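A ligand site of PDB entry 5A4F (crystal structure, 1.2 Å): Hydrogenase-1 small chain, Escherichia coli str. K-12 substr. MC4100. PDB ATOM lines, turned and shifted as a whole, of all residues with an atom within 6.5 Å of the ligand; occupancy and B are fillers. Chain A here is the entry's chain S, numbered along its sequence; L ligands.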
ATOM      1  N   ILE A 186      17.298  -2.762  27.107  1.00  0.00           N
ATOM      2  CA  ILE A 186      16.157  -3.512  26.605  1.00  0.00           C
ATOM      3  C   ILE A 186      16.126  -3.562  25.083  1.00  0.00           C
ATOM      4  O   ILE A 186      15.942  -4.623  24.478  1.00  0.00           O
ATOM      5  CB  ILE A 186      14.806  -2.898  27.149  1.00  0.00           C
ATOM      6  CG1 ILE A 186      14.647  -3.010  28.669  1.00  0.00           C
ATOM      7  CG2 ILE A 186      13.582  -3.420  26.414  1.00  0.00           C
ATOM      8  CD1 ILE A 186      14.505  -4.390  29.164  1.00  0.00           C
ATOM      9  N   HIS A 187      16.380  -2.424  24.470  1.00  0.00           N
ATOM     10  CA  HIS A 187      16.324  -2.254  22.993  1.00  0.00           C
ATOM     11  C   HIS A 187      17.461  -2.984  22.283  1.00  0.00           C
ATOM     12  O   HIS A 187      17.339  -3.240  21.079  1.00  0.00           O
ATOM     13  CB  HIS A 187      16.360  -0.734  22.759  1.00  0.00           C
ATOM     14  CG  HIS A 187      16.375  -0.232  21.354  1.00  0.00           C
ATOM     15  ND1 HIS A 187      15.256  -0.206  20.553  1.00  0.00           N
ATOM     16  CD2 HIS A 187      17.333   0.452  20.689  1.00  0.00           C
ATOM     17  CE1 HIS A 187      15.551   0.401  19.420  1.00  0.00           C
ATOM     18  NE2 HIS A 187      16.797   0.831  19.490  1.00  0.00           N
ATOM     19  N   ASP A 188      18.541  -3.327  23.020  1.00  0.00           N
ATOM     20  CA  ASP A 188      19.659  -4.074  22.439  1.00  0.00           C
ATOM     21  C   ASP A 188      19.445  -5.565  22.423  1.00  0.00           C
ATOM     22  O   ASP A 188      20.251  -6.282  21.784  1.00  0.00           O
ATOM     23  CB  ASP A 188      20.916  -3.622  23.077  1.00  0.00           C
ATOM     24  CG  ASP A 188      21.245  -2.109  22.601  1.00  0.00           C
ATOM     25  OD1 ASP A 188      20.700  -1.591  21.538  1.00  0.00           O
ATOM     26  OD2 ASP A 188      22.008  -1.474  23.217  1.00  0.00           O
ATOM     27  N   CYS A 190      15.840  -6.607  22.051  1.00  0.00           N
ATOM     28  CA  CYS A 190      14.396  -6.668  21.824  1.00  0.00           C
ATOM     29  C   CYS A 190      14.046  -7.388  20.537  1.00  0.00           C
ATOM     30  O   CYS A 190      14.568  -7.070  19.455  1.00  0.00           O
ATOM     31  CB  CYS A 190      13.830  -5.255  21.788  1.00  0.00           C
ATOM     32  SG  CYS A 190      12.004  -5.202  21.586  1.00  0.00           S
ATOM     33  N   TYR A 191      13.118  -8.323  20.640  1.00  0.00           N
ATOM     34  CA  TYR A 191      12.707  -9.111  19.479  1.00  0.00           C
ATOM     35  C   TYR A 191      11.935  -8.283  18.453  1.00  0.00           C
ATOM     36  O   TYR A 191      11.723  -8.803  17.347  1.00  0.00           O
ATOM     37  CB  TYR A 191      11.910 -10.367  19.949  1.00  0.00           C
ATOM     38  CG  TYR A 191      10.449 -10.130  20.214  1.00  0.00           C
ATOM     39  CD1 TYR A 191       9.992  -9.183  21.143  1.00  0.00           C
ATOM     40  CD2 TYR A 191       9.502 -10.906  19.572  1.00  0.00           C
ATOM     41  CE1 TYR A 191       8.629  -9.012  21.380  1.00  0.00           C
ATOM     42  CE2 TYR A 191       8.152 -10.716  19.774  1.00  0.00           C
ATOM     43  CZ  TYR A 191       7.712  -9.744  20.661  1.00  0.00           C
ATOM     44  OH  TYR A 191       6.365  -9.482  20.857  1.00  0.00           O
ATOM     45  N   ARG A 192      11.529  -7.039  18.737  1.00  0.00           N
ATOM     46  CA  ARG A 192      10.889  -6.197  17.727  1.00  0.00           C
ATOM     47  C   ARG A 192      11.893  -5.270  17.072  1.00  0.00           C
ATOM     48  O   ARG A 192      11.472  -4.421  16.252  1.00  0.00           O
ATOM     49  CB  ARG A 192       9.708  -5.396  18.333  1.00  0.00           C
ATOM     50  CG  ARG A 192       8.592  -6.297  18.847  1.00  0.00           C
ATOM     51  CD  ARG A 192       7.397  -5.552  19.320  1.00  0.00           C
ATOM     52  NE  ARG A 192       6.392  -6.436  19.888  1.00  0.00           N
ATOM     53  CZ  ARG A 192       5.092  -6.226  19.970  1.00  0.00           C
ATOM     54  NH1 ARG A 192       4.543  -5.118  19.500  1.00  0.00           N
ATOM     55  NH2 ARG A 192       4.286  -7.151  20.549  1.00  0.00           N
ATOM     56  N   ARG A 193      13.169  -5.417  17.330  1.00  0.00           N
ATOM     57  CA  ARG A 193      14.173  -4.511  16.768  1.00  0.00           C
ATOM     58  C   ARG A 193      14.182  -4.546  15.242  1.00  0.00           C
ATOM     59  O   ARG A 193      14.442  -3.509  14.610  1.00  0.00           O
ATOM     60  CB  ARG A 193      15.548  -4.832  17.328  1.00  0.00           C
ATOM     61  CG  ARG A 193      16.633  -3.903  16.915  1.00  0.00           C
ATOM     62  CD  ARG A 193      16.449  -2.451  17.419  1.00  0.00           C
ATOM     63  NE  ARG A 193      17.597  -1.734  16.899  1.00  0.00           N
ATOM     64  CZ  ARG A 193      18.723  -1.511  17.557  1.00  0.00           C
ATOM     65  NH1 ARG A 193      18.880  -1.791  18.850  1.00  0.00           N
ATOM     66  NH2 ARG A 193      19.727  -0.963  16.915  1.00  0.00           N
ATOM     67  N   ALA A 194      13.912  -5.700  14.638  1.00  0.00           N
ATOM     68  CA  ALA A 194      13.853  -5.760  13.181  1.00  0.00           C
ATOM     69  C   ALA A 194      12.878  -4.724  12.640  1.00  0.00           C
ATOM     70  O   ALA A 194      13.110  -4.092  11.600  1.00  0.00           O
ATOM     71  CB  ALA A 194      13.381  -7.109  12.727  1.00  0.00           C
ATOM     72  N   HIS A 195      11.746  -4.576  13.337  1.00  0.00           N
ATOM     73  CA  HIS A 195      10.724  -3.611  12.915  1.00  0.00           C
ATOM     74  C   HIS A 195      11.175  -2.145  13.117  1.00  0.00           C
ATOM     75  O   HIS A 195      10.999  -1.301  12.216  1.00  0.00           O
ATOM     76  CB  HIS A 195       9.415  -3.857  13.623  1.00  0.00           C
ATOM     77  CG  HIS A 195       8.881  -5.231  13.389  1.00  0.00           C
ATOM     78  ND1 HIS A 195       8.658  -5.735  12.128  1.00  0.00           N
ATOM     79  CD2 HIS A 195       8.547  -6.219  14.243  1.00  0.00           C
ATOM     80  CE1 HIS A 195       8.181  -6.968  12.215  1.00  0.00           C
ATOM     81  NE2 HIS A 195       8.092  -7.278  13.501  1.00  0.00           N
ATOM     82  N   PHE A 196      11.794  -1.879  14.235  1.00  0.00           N
ATOM     83  CA  PHE A 196      12.419  -0.563  14.477  1.00  0.00           C
ATOM     84  C   PHE A 196      13.355  -0.221  13.294  1.00  0.00           C
ATOM     85  O   PHE A 196      13.319   0.873  12.742  1.00  0.00           O
ATOM     86  CB  PHE A 196      13.186  -0.586  15.781  1.00  0.00           C
ATOM     87  CG  PHE A 196      13.919   0.705  16.112  1.00  0.00           C
ATOM     88  CD1 PHE A 196      13.272   1.726  16.827  1.00  0.00           C
ATOM     89  CD2 PHE A 196      15.220   0.888  15.739  1.00  0.00           C
ATOM     90  CE1 PHE A 196      13.950   2.918  17.145  1.00  0.00           C
ATOM     91  CE2 PHE A 196      15.908   2.044  16.090  1.00  0.00           C
ATOM     92  CZ  PHE A 196      15.293   3.052  16.785  1.00  0.00           C
ATOM     93  N   PHE A 201       6.262   0.544  12.534  1.00  0.00           N
ATOM     94  CA  PHE A 201       5.846   1.026  13.842  1.00  0.00           C
ATOM     95  C   PHE A 201       4.336   0.927  14.014  1.00  0.00           C
ATOM     96  O   PHE A 201       3.552   1.227  13.098  1.00  0.00           O
ATOM     97  CB  PHE A 201       6.213   2.485  14.006  1.00  0.00           C
ATOM     98  CG  PHE A 201       7.692   2.769  13.937  1.00  0.00           C
ATOM     99  CD1 PHE A 201       8.537   2.280  14.914  1.00  0.00           C
ATOM    100  CD2 PHE A 201       8.267   3.515  12.884  1.00  0.00           C
ATOM    101  CE1 PHE A 201       9.886   2.492  14.869  1.00  0.00           C
ATOM    102  CE2 PHE A 201       9.599   3.759  12.875  1.00  0.00           C
ATOM    103  CZ  PHE A 201      10.436   3.271  13.848  1.00  0.00           C
ATOM    104  N   TYR A 214       4.634  -5.032  15.527  1.00  0.00           N
ATOM    105  CA  TYR A 214       5.596  -4.032  15.143  1.00  0.00           C
ATOM    106  C   TYR A 214       6.091  -3.236  16.342  1.00  0.00           C
ATOM    107  O   TYR A 214       5.629  -3.356  17.479  1.00  0.00           O
ATOM    108  CB  TYR A 214       4.990  -3.117  14.056  1.00  0.00           C
ATOM    109  CG  TYR A 214       4.951  -3.703  12.638  1.00  0.00           C
ATOM    110  CD1 TYR A 214       5.220  -5.032  12.342  1.00  0.00           C
ATOM    111  CD2 TYR A 214       4.559  -2.867  11.582  1.00  0.00           C
ATOM    112  CE1 TYR A 214       5.178  -5.524  11.035  1.00  0.00           C
ATOM    113  CE2 TYR A 214       4.478  -3.353  10.302  1.00  0.00           C
ATOM    114  CZ  TYR A 214       4.751  -4.682  10.041  1.00  0.00           C
ATOM    115  OH  TYR A 214       4.698  -5.165   8.736  1.00  0.00           O
ATOM    116  N   CYS A 215       7.151  -2.482  16.103  1.00  0.00           N
ATOM    117  CA  CYS A 215       7.878  -1.754  17.147  1.00  0.00           C
ATOM    118  C   CYS A 215       6.990  -0.643  17.758  1.00  0.00           C
ATOM    119  O   CYS A 215       6.127  -0.064  17.056  1.00  0.00           O
ATOM    120  CB  CYS A 215       9.179  -1.198  16.559  1.00  0.00           C
ATOM    121  SG  CYS A 215      10.043   0.016  17.625  1.00  0.00           S
ATOM    122  N   LEU A 216       7.163  -0.481  19.049  1.00  0.00           N
ATOM    123  CA  LEU A 216       6.418   0.449  19.905  1.00  0.00           C
ATOM    124  C   LEU A 216       7.081   1.801  20.133  1.00  0.00           C
ATOM    125  O   LEU A 216       6.578   2.605  20.960  1.00  0.00           O
ATOM    126  CB  LEU A 216       6.057  -0.240  21.229  1.00  0.00           C
ATOM    127  CG  LEU A 216       5.266  -1.492  21.008  1.00  0.00           C
ATOM    128  CD1 LEU A 216       5.137  -2.327  22.274  1.00  0.00           C
ATOM    129  CD2 LEU A 216       3.845  -1.228  20.550  1.00  0.00           C
ATOM    130  N   TYR A 217       8.143   2.109  19.384  1.00  0.00           N
ATOM    131  CA  TYR A 217       8.850   3.375  19.572  1.00  0.00           C
ATOM    132  C   TYR A 217       7.941   4.609  19.433  1.00  0.00           C
ATOM    133  O   TYR A 217       8.012   5.539  20.255  1.00  0.00           O
ATOM    134  CB  TYR A 217       9.965   3.437  18.543  1.00  0.00           C
ATOM    135  CG  TYR A 217      10.619   4.783  18.464  1.00  0.00           C
ATOM    136  CD1 TYR A 217      11.471   5.203  19.446  1.00  0.00           C
ATOM    137  CD2 TYR A 217      10.340   5.607  17.352  1.00  0.00           C
ATOM    138  CE1 TYR A 217      12.086   6.441  19.324  1.00  0.00           C
ATOM    139  CE2 TYR A 217      10.927   6.821  17.231  1.00  0.00           C
ATOM    140  CZ  TYR A 217      11.770   7.250  18.232  1.00  0.00           C
ATOM    141  OH  TYR A 217      12.285   8.425  18.083  1.00  0.00           O
ATOM    142  N   LYS A 218       7.066   4.608  18.429  1.00  0.00           N
ATOM    143  CA  LYS A 218       6.177   5.760  18.252  1.00  0.00           C
ATOM    144  C   LYS A 218       5.047   5.829  19.244  1.00  0.00           C
ATOM    145  O   LYS A 218       4.378   6.873  19.382  1.00  0.00           O
ATOM    146  CB  LYS A 218       5.630   5.853  16.813  1.00  0.00           C
ATOM    147  CG  LYS A 218       6.706   6.072  15.755  1.00  0.00           C
ATOM    148  CD  LYS A 218       6.134   6.385  14.379  1.00  0.00           C
ATOM    149  CE  LYS A 218       7.297   6.812  13.471  1.00  0.00           C
ATOM    150  NZ  LYS A 218       6.802   7.119  12.082  1.00  0.00           N
ATOM    151  N   CYS A 221       7.750   3.802  23.656  1.00  0.00           N
ATOM    152  CA  CYS A 221       8.655   2.828  24.274  1.00  0.00           C
ATOM    153  C   CYS A 221       9.966   3.471  24.695  1.00  0.00           C
ATOM    154  O   CYS A 221      10.668   4.076  23.884  1.00  0.00           O
ATOM    155  CB  CYS A 221       8.939   1.717  23.255  1.00  0.00           C
ATOM    156  SG  CYS A 221       9.889   0.371  23.992  1.00  0.00           S
ATOM    157  N   LYS A 222      10.342   3.248  25.951  1.00  0.00           N
ATOM    158  CA  LYS A 222      11.581   3.731  26.510  1.00  0.00           C
ATOM    159  C   LYS A 222      12.668   2.690  26.577  1.00  0.00           C
ATOM    160  O   LYS A 222      13.748   2.877  27.165  1.00  0.00           O
ATOM    161  CB  LYS A 222      11.352   4.376  27.884  1.00  0.00           C
ATOM    162  CG  LYS A 222      10.349   5.554  27.810  1.00  0.00           C
ATOM    163  CD  LYS A 222      10.666   6.544  26.686  1.00  0.00           C
ATOM    164  CE  LYS A 222       9.874   7.816  26.658  1.00  0.00           C
ATOM    165  NZ  LYS A 222       8.411   7.644  26.790  1.00  0.00           N
ATOM    166  N   GLY A 223      12.453   1.584  25.853  1.00  0.00           N
ATOM    167  CA  GLY A 223      13.466   0.554  25.730  1.00  0.00           C
ATOM    168  C   GLY A 223      14.860   1.023  25.301  1.00  0.00           C
ATOM    169  O   GLY A 223      15.883   0.560  25.822  1.00  0.00           O
ATOM    170  N   PRO A 224      14.932   2.033  24.402  1.00  0.00           N
ATOM    171  CA  PRO A 224      16.256   2.499  23.949  1.00  0.00           C
ATOM    172  C   PRO A 224      17.141   3.114  25.029  1.00  0.00           C
ATOM    173  O   PRO A 224      18.355   3.248  24.833  1.00  0.00           O
ATOM    174  CB  PRO A 224      15.889   3.546  22.871  1.00  0.00           C
ATOM    175  CG  PRO A 224      14.634   3.000  22.301  1.00  0.00           C
ATOM    176  CD  PRO A 224      13.873   2.522  23.507  1.00  0.00           C
ATOM    177  N   PHE A 241       6.814  -9.999  28.469  1.00  0.00           N
ATOM    178  CA  PHE A 241       7.346  -8.802  29.038  1.00  0.00           C
ATOM    179  C   PHE A 241       6.514  -7.669  28.479  1.00  0.00           C
ATOM    180  O   PHE A 241       5.701  -7.873  27.571  1.00  0.00           O
ATOM    181  CB  PHE A 241       8.861  -8.625  28.837  1.00  0.00           C
ATOM    182  CG  PHE A 241       9.353  -8.239  27.446  1.00  0.00           C
ATOM    183  CD1 PHE A 241       9.313  -9.125  26.383  1.00  0.00           C
ATOM    184  CD2 PHE A 241      10.009  -7.023  27.267  1.00  0.00           C
ATOM    185  CE1 PHE A 241       9.868  -8.777  25.131  1.00  0.00           C
ATOM    186  CE2 PHE A 241      10.546  -6.722  26.032  1.00  0.00           C
ATOM    187  CZ  PHE A 241      10.449  -7.612  24.987  1.00  0.00           C
ATOM    188  N   ILE A 243       6.680  -5.166  26.319  1.00  0.00           N
ATOM    189  CA  ILE A 243       6.656  -4.994  24.868  1.00  0.00           C
ATOM    190  C   ILE A 243       6.026  -6.182  24.169  1.00  0.00           C
ATOM    191  O   ILE A 243       5.248  -5.984  23.234  1.00  0.00           O
ATOM    192  CB  ILE A 243       8.070  -4.716  24.388  1.00  0.00           C
ATOM    193  CG1 ILE A 243       8.544  -3.345  24.784  1.00  0.00           C
ATOM    194  CG2 ILE A 243       8.256  -4.931  22.890  1.00  0.00           C
ATOM    195  CD1 ILE A 243      10.018  -3.225  25.079  1.00  0.00           C
ATOM    196  N   GLY A 248       4.726  -0.227  25.230  1.00  0.00           N
ATOM    197  CA  GLY A 248       6.103   0.160  25.306  1.00  0.00           C
ATOM    198  C   GLY A 248       6.652   0.073  26.704  1.00  0.00           C
ATOM    199  O   GLY A 248       5.914   0.228  27.690  1.00  0.00           O
ATOM    200  N   CYS A 249       7.943  -0.127  26.821  1.00  0.00           N
ATOM    201  CA  CYS A 249       8.659   0.016  28.079  1.00  0.00           C
ATOM    202  C   CYS A 249       8.371   1.413  28.644  1.00  0.00           C
ATOM    203  O   CYS A 249       8.403   2.423  27.893  1.00  0.00           O
ATOM    204  CB  CYS A 249      10.152  -0.206  27.823  1.00  0.00           C
ATOM    205  SG  CYS A 249      11.272   0.006  29.230  1.00  0.00           S
HETATM  206 FE1  LIG L   1      10.963  -0.978  19.453  1.00  0.00          FE
HETATM  207 FE2  LIG L   1      10.899  -0.600  22.172  1.00  0.00          FE
HETATM  208 FE3  LIG L   1      13.275  -0.800  20.832  1.00  0.00          FE
HETATM  209 FE4  LIG L   1      11.728  -2.985  21.122  1.00  0.00          FE
HETATM  210  S1  LIG L   1      12.758  -1.782  22.822  1.00  0.00           S
HETATM  211  S2  LIG L   1      12.767  -2.347  19.184  1.00  0.00           S
HETATM  212  S3  LIG L   1       9.625  -2.076  20.931  1.00  0.00           S
HETATM  213  S4  LIG L   1      11.726   0.878  20.652  1.00  0.00           S
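The side-chain sulfur of Cys 190 lies close to the backbone NH of Arg 192 (3.4 Å).
NH1 of Arg 193 sits at hydrogen-bond distance from O of His 187, at 3.1 Å.
NH1 of Arg 193 is in salt-bridge range of OD1 of Asp 188, 3.3 Å away.
SG of Cys 215 lies close to N of Tyr 217, at 3.3 Å.
N of His 187 is in hydrogen-bond range of O of Gly 223 (3.3 Å).
The side-chain sulfur of Cys 221 sits close to the backbone NH of Gly 223.
NH1 of Arg 192 lies within hydrogen-bond range of O of Tyr 214, at 2.9 Å.
The side-chain sulfur (SG) of Cys 221 lies close to the backbone NH (N) of Cys 249, 3.5 Å away.
Arg 192 touches the ligand.
CB of Phe 196 touches S2 of the ligand, at 3.9 Å.
Tyr 217 touches the ligand (CB to S4, 3.8 Å).
Gly 223 touches the ligand (CA to S1, 3.8 Å).
CD of Pro 224 touches S4 of the ligand (3.9 Å).
Ile 243 touches the ligand (CG2 to S3, 3.7 Å).
Hydrophobic or aromatic side chains within 4 Å of the ligand: His 187, Phe 196, Tyr 217, Pro 224 and Ile 243.
Within 4 Å of the ligand: His 187, Cys 190, Arg 192, Arg 193, Phe 196, Cys 215, Leu 216, Tyr 217, Cys 221, Gly 223, Pro 224 and Ile 243.
The backbone NH of Arg 193 lies close to a sulfur (S2) of the ligand (3.6 Å).
S3 of the ligand sits close to N of Leu 216.
FE1 of the ligand is bound by SG of Cys 215 (2.3 Å).
FE3 of the ligand is bound by ND1 of His 187.
SG of Cys 190 binds FE4 of the ligand, at 2.3 Å.
SG of Cys 221 is bound to FE2 of the ligand.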
